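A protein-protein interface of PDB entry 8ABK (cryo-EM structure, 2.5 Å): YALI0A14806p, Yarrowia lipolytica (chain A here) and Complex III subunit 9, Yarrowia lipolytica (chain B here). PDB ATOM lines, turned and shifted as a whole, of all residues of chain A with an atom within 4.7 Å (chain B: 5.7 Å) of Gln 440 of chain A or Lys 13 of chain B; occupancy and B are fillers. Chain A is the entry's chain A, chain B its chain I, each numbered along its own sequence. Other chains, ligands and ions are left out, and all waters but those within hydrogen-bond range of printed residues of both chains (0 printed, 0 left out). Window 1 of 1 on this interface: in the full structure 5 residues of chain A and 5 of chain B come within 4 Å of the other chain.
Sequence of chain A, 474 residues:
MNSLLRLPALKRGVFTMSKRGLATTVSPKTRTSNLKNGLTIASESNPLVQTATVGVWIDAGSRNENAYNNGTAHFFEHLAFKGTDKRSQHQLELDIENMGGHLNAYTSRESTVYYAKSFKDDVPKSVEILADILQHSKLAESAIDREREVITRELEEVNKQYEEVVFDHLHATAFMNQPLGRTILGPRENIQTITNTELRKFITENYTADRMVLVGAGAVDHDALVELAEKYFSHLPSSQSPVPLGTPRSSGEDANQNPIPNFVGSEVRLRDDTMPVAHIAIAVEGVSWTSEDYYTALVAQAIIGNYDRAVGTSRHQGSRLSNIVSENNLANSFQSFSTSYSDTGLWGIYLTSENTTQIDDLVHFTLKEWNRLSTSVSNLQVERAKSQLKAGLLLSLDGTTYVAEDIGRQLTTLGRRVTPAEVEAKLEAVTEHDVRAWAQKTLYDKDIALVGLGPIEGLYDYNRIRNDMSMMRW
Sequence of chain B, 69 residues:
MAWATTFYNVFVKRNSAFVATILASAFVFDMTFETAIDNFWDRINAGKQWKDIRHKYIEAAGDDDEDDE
The backbone carbonyl oxygen of Trp 474 of chain A sits close to the backbone NH of Asn 15 of chain B, at 3.3 Å. The side-chain amino group of Lys 13 of chain B lies within hydrogen-bond range of the side-chain amide oxygen of Gln 440 of chain A, at 2.9 Å.
The backbone carbonyl oxygen (O) of Ser 374 of chain A is in hydrogen-bond range of the side-chain amide nitrogen (NE2) of Gln 440 of chain A. The backbone carbonyl oxygen (O) of Tyr 8 of chain B is in hydrogen-bond range of the backbone NH (N) of Lys 13 of chain B (2.8 Å). The guanidinium group of Arg 14 of chain B is in hydrogen-bond range of the backbone carbonyl oxygen of Asn 9 of chain B, at 3.2 Å. O of Ala 439 of chain A lies within hydrogen-bond range of N of Tyr 444 of chain A (2.9 Å). The side-chain amide oxygen of Asn 9 of chain B lies within hydrogen-bond range of the side-chain amino group of Lys 13 of chain B (3.2 Å).
Among the printed residues, pairs that only touch across the chains: Tyr 444 of chain A with Lys 13 of chain B (3.5 Å), Trp 474 of chain A with Arg 14 of chain B (3.7 Å) and Trp 474 of chain A with Lys 13 of chain B (3.9 Å).
Gln 440 of chain A touches one residue of chain B. Of chain A, only Gln 440 (2.9 Å), Tyr 444 (3.5 Å) and Trp 474 (3.9 Å) come within 4 Å of Lys 13 of chain B. Of the printed residues of chain B, Tyr 444 of chain A touches Lys 13. Of the printed residues of chain B, Trp 474 of chain A touches Lys 13 (3.9 Å), Arg 14 (3.7 Å) and Asn 15 (3.3 Å). Of the printed residues of chain A, Arg 14 of chain B touches Trp 474 (3.7 Å). Printed residues of chain A within 4 Å of Asn 15 of chain B: Trp 474 (3.3 Å). The nearest printed residue of chain A that does not touch Lys 13 of chain B is Lys 441 of chain A (5.9 Å). The nearest printed residue of chain A that does not touch Arg 14 of chain B is Gln 440 of chain A (4.1 Å).
Of the 10 printed residues of chain A, 3 touch a printed residue of chain B. Hydrophobic or aromatic side chains of chain A that line the printed part of chain B: Tyr 444 and Trp 474. Among the printed residues, 5 pairs touch across the chains.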
ATOM      1  N   SER A 374      30.766 -17.143  -5.481  1.00  0.00           N
ATOM      2  CA  SER A 374      30.850 -15.720  -5.762  1.00  0.00           C
ATOM      3  C   SER A 374      31.779 -15.029  -4.771  1.00  0.00           C
ATOM      4  O   SER A 374      32.453 -14.075  -5.141  1.00  0.00           O
ATOM      5  CB  SER A 374      29.503 -15.045  -5.746  1.00  0.00           C
ATOM      6  OG  SER A 374      28.622 -15.585  -6.722  1.00  0.00           O
ATOM      7  N   ARG A 436      34.671 -16.818 -10.083  1.00  0.00           N
ATOM      8  CA  ARG A 436      33.993 -15.781  -9.309  1.00  0.00           C
ATOM      9  C   ARG A 436      33.179 -14.878 -10.238  1.00  0.00           C
ATOM     10  O   ARG A 436      32.036 -14.544  -9.940  1.00  0.00           O
ATOM     11  CB  ARG A 436      34.947 -14.925  -8.463  1.00  0.00           C
ATOM     12  CG  ARG A 436      35.583 -15.621  -7.266  1.00  0.00           C
ATOM     13  CD  ARG A 436      36.874 -14.945  -6.793  1.00  0.00           C
ATOM     14  NE  ARG A 436      36.440 -13.724  -6.152  1.00  0.00           N
ATOM     15  CZ  ARG A 436      35.955 -13.667  -4.915  1.00  0.00           C
ATOM     16  NH1 ARG A 436      35.908 -14.752  -4.156  1.00  0.00           N
ATOM     17  NH2 ARG A 436      35.529 -12.517  -4.428  1.00  0.00           N
ATOM     18  N   ALA A 437      33.766 -14.471 -11.364  1.00  0.00           N
ATOM     19  CA  ALA A 437      33.056 -13.562 -12.244  1.00  0.00           C
ATOM     20  C   ALA A 437      31.800 -14.226 -12.802  1.00  0.00           C
ATOM     21  O   ALA A 437      30.771 -13.566 -12.931  1.00  0.00           O
ATOM     22  CB  ALA A 437      33.968 -13.096 -13.341  1.00  0.00           C
ATOM     23  N   TRP A 438      31.900 -15.517 -13.143  1.00  0.00           N
ATOM     24  CA  TRP A 438      30.775 -16.254 -13.693  1.00  0.00           C
ATOM     25  C   TRP A 438      29.670 -16.377 -12.644  1.00  0.00           C
ATOM     26  O   TRP A 438      28.503 -16.152 -12.955  1.00  0.00           O
ATOM     27  CB  TRP A 438      31.227 -17.614 -14.241  1.00  0.00           C
ATOM     28  CG  TRP A 438      30.083 -18.443 -14.727  1.00  0.00           C
ATOM     29  CD1 TRP A 438      29.492 -18.403 -15.958  1.00  0.00           C
ATOM     30  CD2 TRP A 438      29.382 -19.429 -13.959  1.00  0.00           C
ATOM     31  NE1 TRP A 438      28.442 -19.282 -15.992  1.00  0.00           N
ATOM     32  CE2 TRP A 438      28.356 -19.927 -14.786  1.00  0.00           C
ATOM     33  CE3 TRP A 438      29.516 -19.919 -12.649  1.00  0.00           C
ATOM     34  CZ2 TRP A 438      27.451 -20.885 -14.334  1.00  0.00           C
ATOM     35  CZ3 TRP A 438      28.626 -20.873 -12.206  1.00  0.00           C
ATOM     36  CH2 TRP A 438      27.612 -21.336 -13.042  1.00  0.00           C
ATOM     37  N   ALA A 439      30.036 -16.746 -11.411  1.00  0.00           N
ATOM     38  CA  ALA A 439      29.030 -16.985 -10.389  1.00  0.00           C
ATOM     39  C   ALA A 439      28.327 -15.676 -10.032  1.00  0.00           C
ATOM     40  O   ALA A 439      27.122 -15.658  -9.766  1.00  0.00           O
ATOM     41  CB  ALA A 439      29.664 -17.642  -9.189  1.00  0.00           C
ATOM     42  N   GLN A 440      29.077 -14.569 -10.096  1.00  0.00           N
ATOM     43  CA  GLN A 440      28.509 -13.278  -9.736  1.00  0.00           C
ATOM     44  C   GLN A 440      27.497 -12.788 -10.766  1.00  0.00           C
ATOM     45  O   GLN A 440      26.603 -12.018 -10.411  1.00  0.00           O
ATOM     46  CB  GLN A 440      29.588 -12.248  -9.484  1.00  0.00           C
ATOM     47  CG  GLN A 440      30.216 -12.496  -8.132  1.00  0.00           C
ATOM     48  CD  GLN A 440      31.408 -11.604  -7.956  1.00  0.00           C
ATOM     49  OE1 GLN A 440      31.534 -10.601  -8.645  1.00  0.00           O
ATOM     50  NE2 GLN A 440      32.295 -11.971  -7.043  1.00  0.00           N
ATOM     51  N   LYS A 441      27.604 -13.250 -12.013  1.00  0.00           N
ATOM     52  CA  LYS A 441      26.609 -12.842 -12.994  1.00  0.00           C
ATOM     53  C   LYS A 441      25.534 -13.899 -13.218  1.00  0.00           C
ATOM     54  O   LYS A 441      24.533 -13.590 -13.846  1.00  0.00           O
ATOM     55  CB  LYS A 441      27.217 -12.405 -14.320  1.00  0.00           C
ATOM     56  CG  LYS A 441      27.926 -13.501 -15.078  1.00  0.00           C
ATOM     57  CD  LYS A 441      28.464 -12.981 -16.359  1.00  0.00           C
ATOM     58  CE  LYS A 441      28.344 -14.022 -17.443  1.00  0.00           C
ATOM     59  NZ  LYS A 441      29.566 -14.052 -18.278  1.00  0.00           N
ATOM     60  N   THR A 442      25.761 -15.132 -12.763  1.00  0.00           N
ATOM     61  CA  THR A 442      24.886 -16.238 -13.115  1.00  0.00           C
ATOM     62  C   THR A 442      24.124 -16.737 -11.899  1.00  0.00           C
ATOM     63  O   THR A 442      22.989 -17.177 -12.034  1.00  0.00           O
ATOM     64  CB  THR A 442      25.687 -17.405 -13.694  1.00  0.00           C
ATOM     65  OG1 THR A 442      26.428 -16.819 -14.760  1.00  0.00           O
ATOM     66  CG2 THR A 442      24.823 -18.528 -14.228  1.00  0.00           C
ATOM     67  N   TYR A 444      24.650 -15.319  -8.342  1.00  0.00           N
ATOM     68  CA  TYR A 444      24.515 -14.463  -7.185  1.00  0.00           C
ATOM     69  C   TYR A 444      23.245 -13.629  -7.298  1.00  0.00           C
ATOM     70  O   TYR A 444      23.083 -12.934  -8.293  1.00  0.00           O
ATOM     71  CB  TYR A 444      25.738 -13.565  -7.023  1.00  0.00           C
ATOM     72  CG  TYR A 444      25.781 -13.059  -5.609  1.00  0.00           C
ATOM     73  CD1 TYR A 444      26.222 -13.897  -4.595  1.00  0.00           C
ATOM     74  CD2 TYR A 444      25.312 -11.795  -5.267  1.00  0.00           C
ATOM     75  CE1 TYR A 444      26.243 -13.483  -3.276  1.00  0.00           C
ATOM     76  CE2 TYR A 444      25.319 -11.364  -3.950  1.00  0.00           C
ATOM     77  CZ  TYR A 444      25.788 -12.212  -2.957  1.00  0.00           C
ATOM     78  OH  TYR A 444      25.806 -11.806  -1.655  1.00  0.00           O
ATOM     79  N   TRP A 474      28.047 -10.082   2.777  1.00  0.00           N
ATOM     80  CA  TRP A 474      28.947  -9.773   1.678  1.00  0.00           C
ATOM     81  C   TRP A 474      28.417  -8.542   0.948  1.00  0.00           C
ATOM     82  O   TRP A 474      29.114  -7.526   1.031  1.00  0.00           O
ATOM     83  CB  TRP A 474      29.107 -10.968   0.728  1.00  0.00           C
ATOM     84  CG  TRP A 474      30.147 -10.828  -0.343  1.00  0.00           C
ATOM     85  CD1 TRP A 474      31.499 -10.966  -0.204  1.00  0.00           C
ATOM     86  CD2 TRP A 474      29.915 -10.629  -1.750  1.00  0.00           C
ATOM     87  NE1 TRP A 474      32.124 -10.834  -1.417  1.00  0.00           N
ATOM     88  CE2 TRP A 474      31.176 -10.639  -2.390  1.00  0.00           C
ATOM     89  CE3 TRP A 474      28.767 -10.447  -2.533  1.00  0.00           C
ATOM     90  CZ2 TRP A 474      31.310 -10.445  -3.771  1.00  0.00           C
ATOM     91  CZ3 TRP A 474      28.892 -10.290  -3.898  1.00  0.00           C
ATOM     92  CH2 TRP A 474      30.153 -10.277  -4.505  1.00  0.00           C
ATOM     93  N   TYR B   8      24.430  -1.868 -10.935  1.00  0.00           N
ATOM     94  CA  TYR B   8      24.119  -2.979 -10.051  1.00  0.00           C
ATOM     95  C   TYR B   8      25.400  -3.533  -9.430  1.00  0.00           C
ATOM     96  O   TYR B   8      25.472  -3.737  -8.218  1.00  0.00           O
ATOM     97  CB  TYR B   8      23.358  -4.091 -10.774  1.00  0.00           C
ATOM     98  CG  TYR B   8      23.145  -5.300  -9.902  1.00  0.00           C
ATOM     99  CD1 TYR B   8      22.080  -5.343  -9.010  1.00  0.00           C
ATOM    100  CD2 TYR B   8      24.033  -6.370  -9.917  1.00  0.00           C
ATOM    101  CE1 TYR B   8      21.872  -6.427  -8.173  1.00  0.00           C
ATOM    102  CE2 TYR B   8      23.852  -7.458  -9.075  1.00  0.00           C
ATOM    103  CZ  TYR B   8      22.759  -7.491  -8.216  1.00  0.00           C
ATOM    104  OH  TYR B   8      22.563  -8.557  -7.390  1.00  0.00           O
ATOM    105  N   ASN B   9      26.411  -3.751 -10.277  1.00  0.00           N
ATOM    106  CA  ASN B   9      27.655  -4.379  -9.864  1.00  0.00           C
ATOM    107  C   ASN B   9      28.424  -3.564  -8.835  1.00  0.00           C
ATOM    108  O   ASN B   9      29.037  -4.138  -7.934  1.00  0.00           O
ATOM    109  CB  ASN B   9      28.532  -4.723 -11.056  1.00  0.00           C
ATOM    110  CG  ASN B   9      28.028  -5.994 -11.685  1.00  0.00           C
ATOM    111  OD1 ASN B   9      27.477  -6.846 -10.991  1.00  0.00           O
ATOM    112  ND2 ASN B   9      28.178  -6.103 -12.989  1.00  0.00           N
ATOM    113  N   VAL B  10      28.382  -2.240  -8.973  1.00  0.00           N
ATOM    114  CA  VAL B  10      29.122  -1.375  -8.080  1.00  0.00           C
ATOM    115  C   VAL B  10      28.333  -1.134  -6.796  1.00  0.00           C
ATOM    116  O   VAL B  10      28.879  -1.275  -5.711  1.00  0.00           O
ATOM    117  CB  VAL B  10      29.537  -0.069  -8.777  1.00  0.00           C
ATOM    118  CG1 VAL B  10      30.176   0.902  -7.799  1.00  0.00           C
ATOM    119  CG2 VAL B  10      30.492  -0.357  -9.922  1.00  0.00           C
ATOM    120  N   PHE B  11      27.051  -0.797  -6.893  1.00  0.00           N
ATOM    121  CA  PHE B  11      26.422  -0.277  -5.694  1.00  0.00           C
ATOM    122  C   PHE B  11      25.454  -1.243  -5.035  1.00  0.00           C
ATOM    123  O   PHE B  11      24.995  -0.971  -3.930  1.00  0.00           O
ATOM    124  CB  PHE B  11      25.611   0.968  -6.023  1.00  0.00           C
ATOM    125  CG  PHE B  11      26.482   2.096  -6.485  1.00  0.00           C
ATOM    126  CD1 PHE B  11      27.248   2.810  -5.576  1.00  0.00           C
ATOM    127  CD2 PHE B  11      26.591   2.388  -7.836  1.00  0.00           C
ATOM    128  CE1 PHE B  11      28.088   3.823  -6.013  1.00  0.00           C
ATOM    129  CE2 PHE B  11      27.423   3.411  -8.269  1.00  0.00           C
ATOM    130  CZ  PHE B  11      28.168   4.124  -7.356  1.00  0.00           C
ATOM    131  N   VAL B  12      25.086  -2.327  -5.714  1.00  0.00           N
ATOM    132  CA  VAL B  12      23.953  -3.093  -5.223  1.00  0.00           C
ATOM    133  C   VAL B  12      24.366  -4.524  -4.900  1.00  0.00           C
ATOM    134  O   VAL B  12      23.975  -5.039  -3.859  1.00  0.00           O
ATOM    135  CB  VAL B  12      22.761  -3.037  -6.192  1.00  0.00           C
ATOM    136  CG1 VAL B  12      21.572  -3.784  -5.621  1.00  0.00           C
ATOM    137  CG2 VAL B  12      22.388  -1.593  -6.497  1.00  0.00           C
ATOM    138  N   LYS B  13      25.168  -5.138  -5.776  1.00  0.00           N
ATOM    139  CA  LYS B  13      25.507  -6.549  -5.672  1.00  0.00           C
ATOM    140  C   LYS B  13      26.064  -6.917  -4.297  1.00  0.00           C
ATOM    141  O   LYS B  13      25.594  -7.863  -3.683  1.00  0.00           O
ATOM    142  CB  LYS B  13      26.509  -6.930  -6.756  1.00  0.00           C
ATOM    143  CG  LYS B  13      27.007  -8.365  -6.691  1.00  0.00           C
ATOM    144  CD  LYS B  13      27.791  -8.772  -7.928  1.00  0.00           C
ATOM    145  CE  LYS B  13      29.111  -8.043  -8.101  1.00  0.00           C
ATOM    146  NZ  LYS B  13      29.766  -8.373  -9.390  1.00  0.00           N
ATOM    147  N   ARG B  14      27.084  -6.213  -3.821  1.00  0.00           N
ATOM    148  CA  ARG B  14      27.612  -6.530  -2.506  1.00  0.00           C
ATOM    149  C   ARG B  14      26.790  -5.760  -1.489  1.00  0.00           C
ATOM    150  O   ARG B  14      26.560  -4.576  -1.687  1.00  0.00           O
ATOM    151  CB  ARG B  14      29.062  -6.076  -2.377  1.00  0.00           C
ATOM    152  CG  ARG B  14      30.023  -6.787  -3.310  1.00  0.00           C
ATOM    153  CD  ARG B  14      31.305  -5.987  -3.390  1.00  0.00           C
ATOM    154  NE  ARG B  14      32.121  -6.751  -4.307  1.00  0.00           N
ATOM    155  CZ  ARG B  14      32.024  -6.692  -5.627  1.00  0.00           C
ATOM    156  NH1 ARG B  14      31.163  -5.870  -6.207  1.00  0.00           N
ATOM    157  NH2 ARG B  14      32.790  -7.467  -6.364  1.00  0.00           N
ATOM    158  N   ASN B  15      26.328  -6.440  -0.436  1.00  0.00           N
ATOM    159  CA  ASN B  15      25.472  -5.806   0.547  1.00  0.00           C
ATOM    160  C   ASN B  15      26.276  -4.760   1.315  1.00  0.00           C
ATOM    161  O   ASN B  15      25.761  -3.709   1.670  1.00  0.00           O
ATOM    162  CB  ASN B  15      24.863  -6.819   1.512  1.00  0.00           C
ATOM    163  CG  ASN B  15      23.684  -6.236   2.255  1.00  0.00           C
ATOM    164  OD1 ASN B  15      22.829  -5.597   1.647  1.00  0.00           O
ATOM    165  ND2 ASN B  15      23.629  -6.428   3.560  1.00  0.00           N
ATOM    166  N   PHE B  18      25.928  -1.836  -0.823  1.00  0.00           N
ATOM    167  CA  PHE B  18      24.543  -1.400  -0.817  1.00  0.00           C
ATOM    168  C   PHE B  18      24.243  -0.633   0.468  1.00  0.00           C
ATOM    169  O   PHE B  18      23.651   0.437   0.402  1.00  0.00           O
ATOM    170  CB  PHE B  18      23.616  -2.599  -1.012  1.00  0.00           C
ATOM    171  CG  PHE B  18      22.164  -2.293  -1.269  1.00  0.00           C
ATOM    172  CD1 PHE B  18      21.790  -1.386  -2.255  1.00  0.00           C
ATOM    173  CD2 PHE B  18      21.167  -2.981  -0.584  1.00  0.00           C
ATOM    174  CE1 PHE B  18      20.448  -1.136  -2.511  1.00  0.00           C
ATOM    175  CE2 PHE B  18      19.824  -2.742  -0.856  1.00  0.00           C
ATOM    176  CZ  PHE B  18      19.467  -1.808  -1.810  1.00  0.00           C
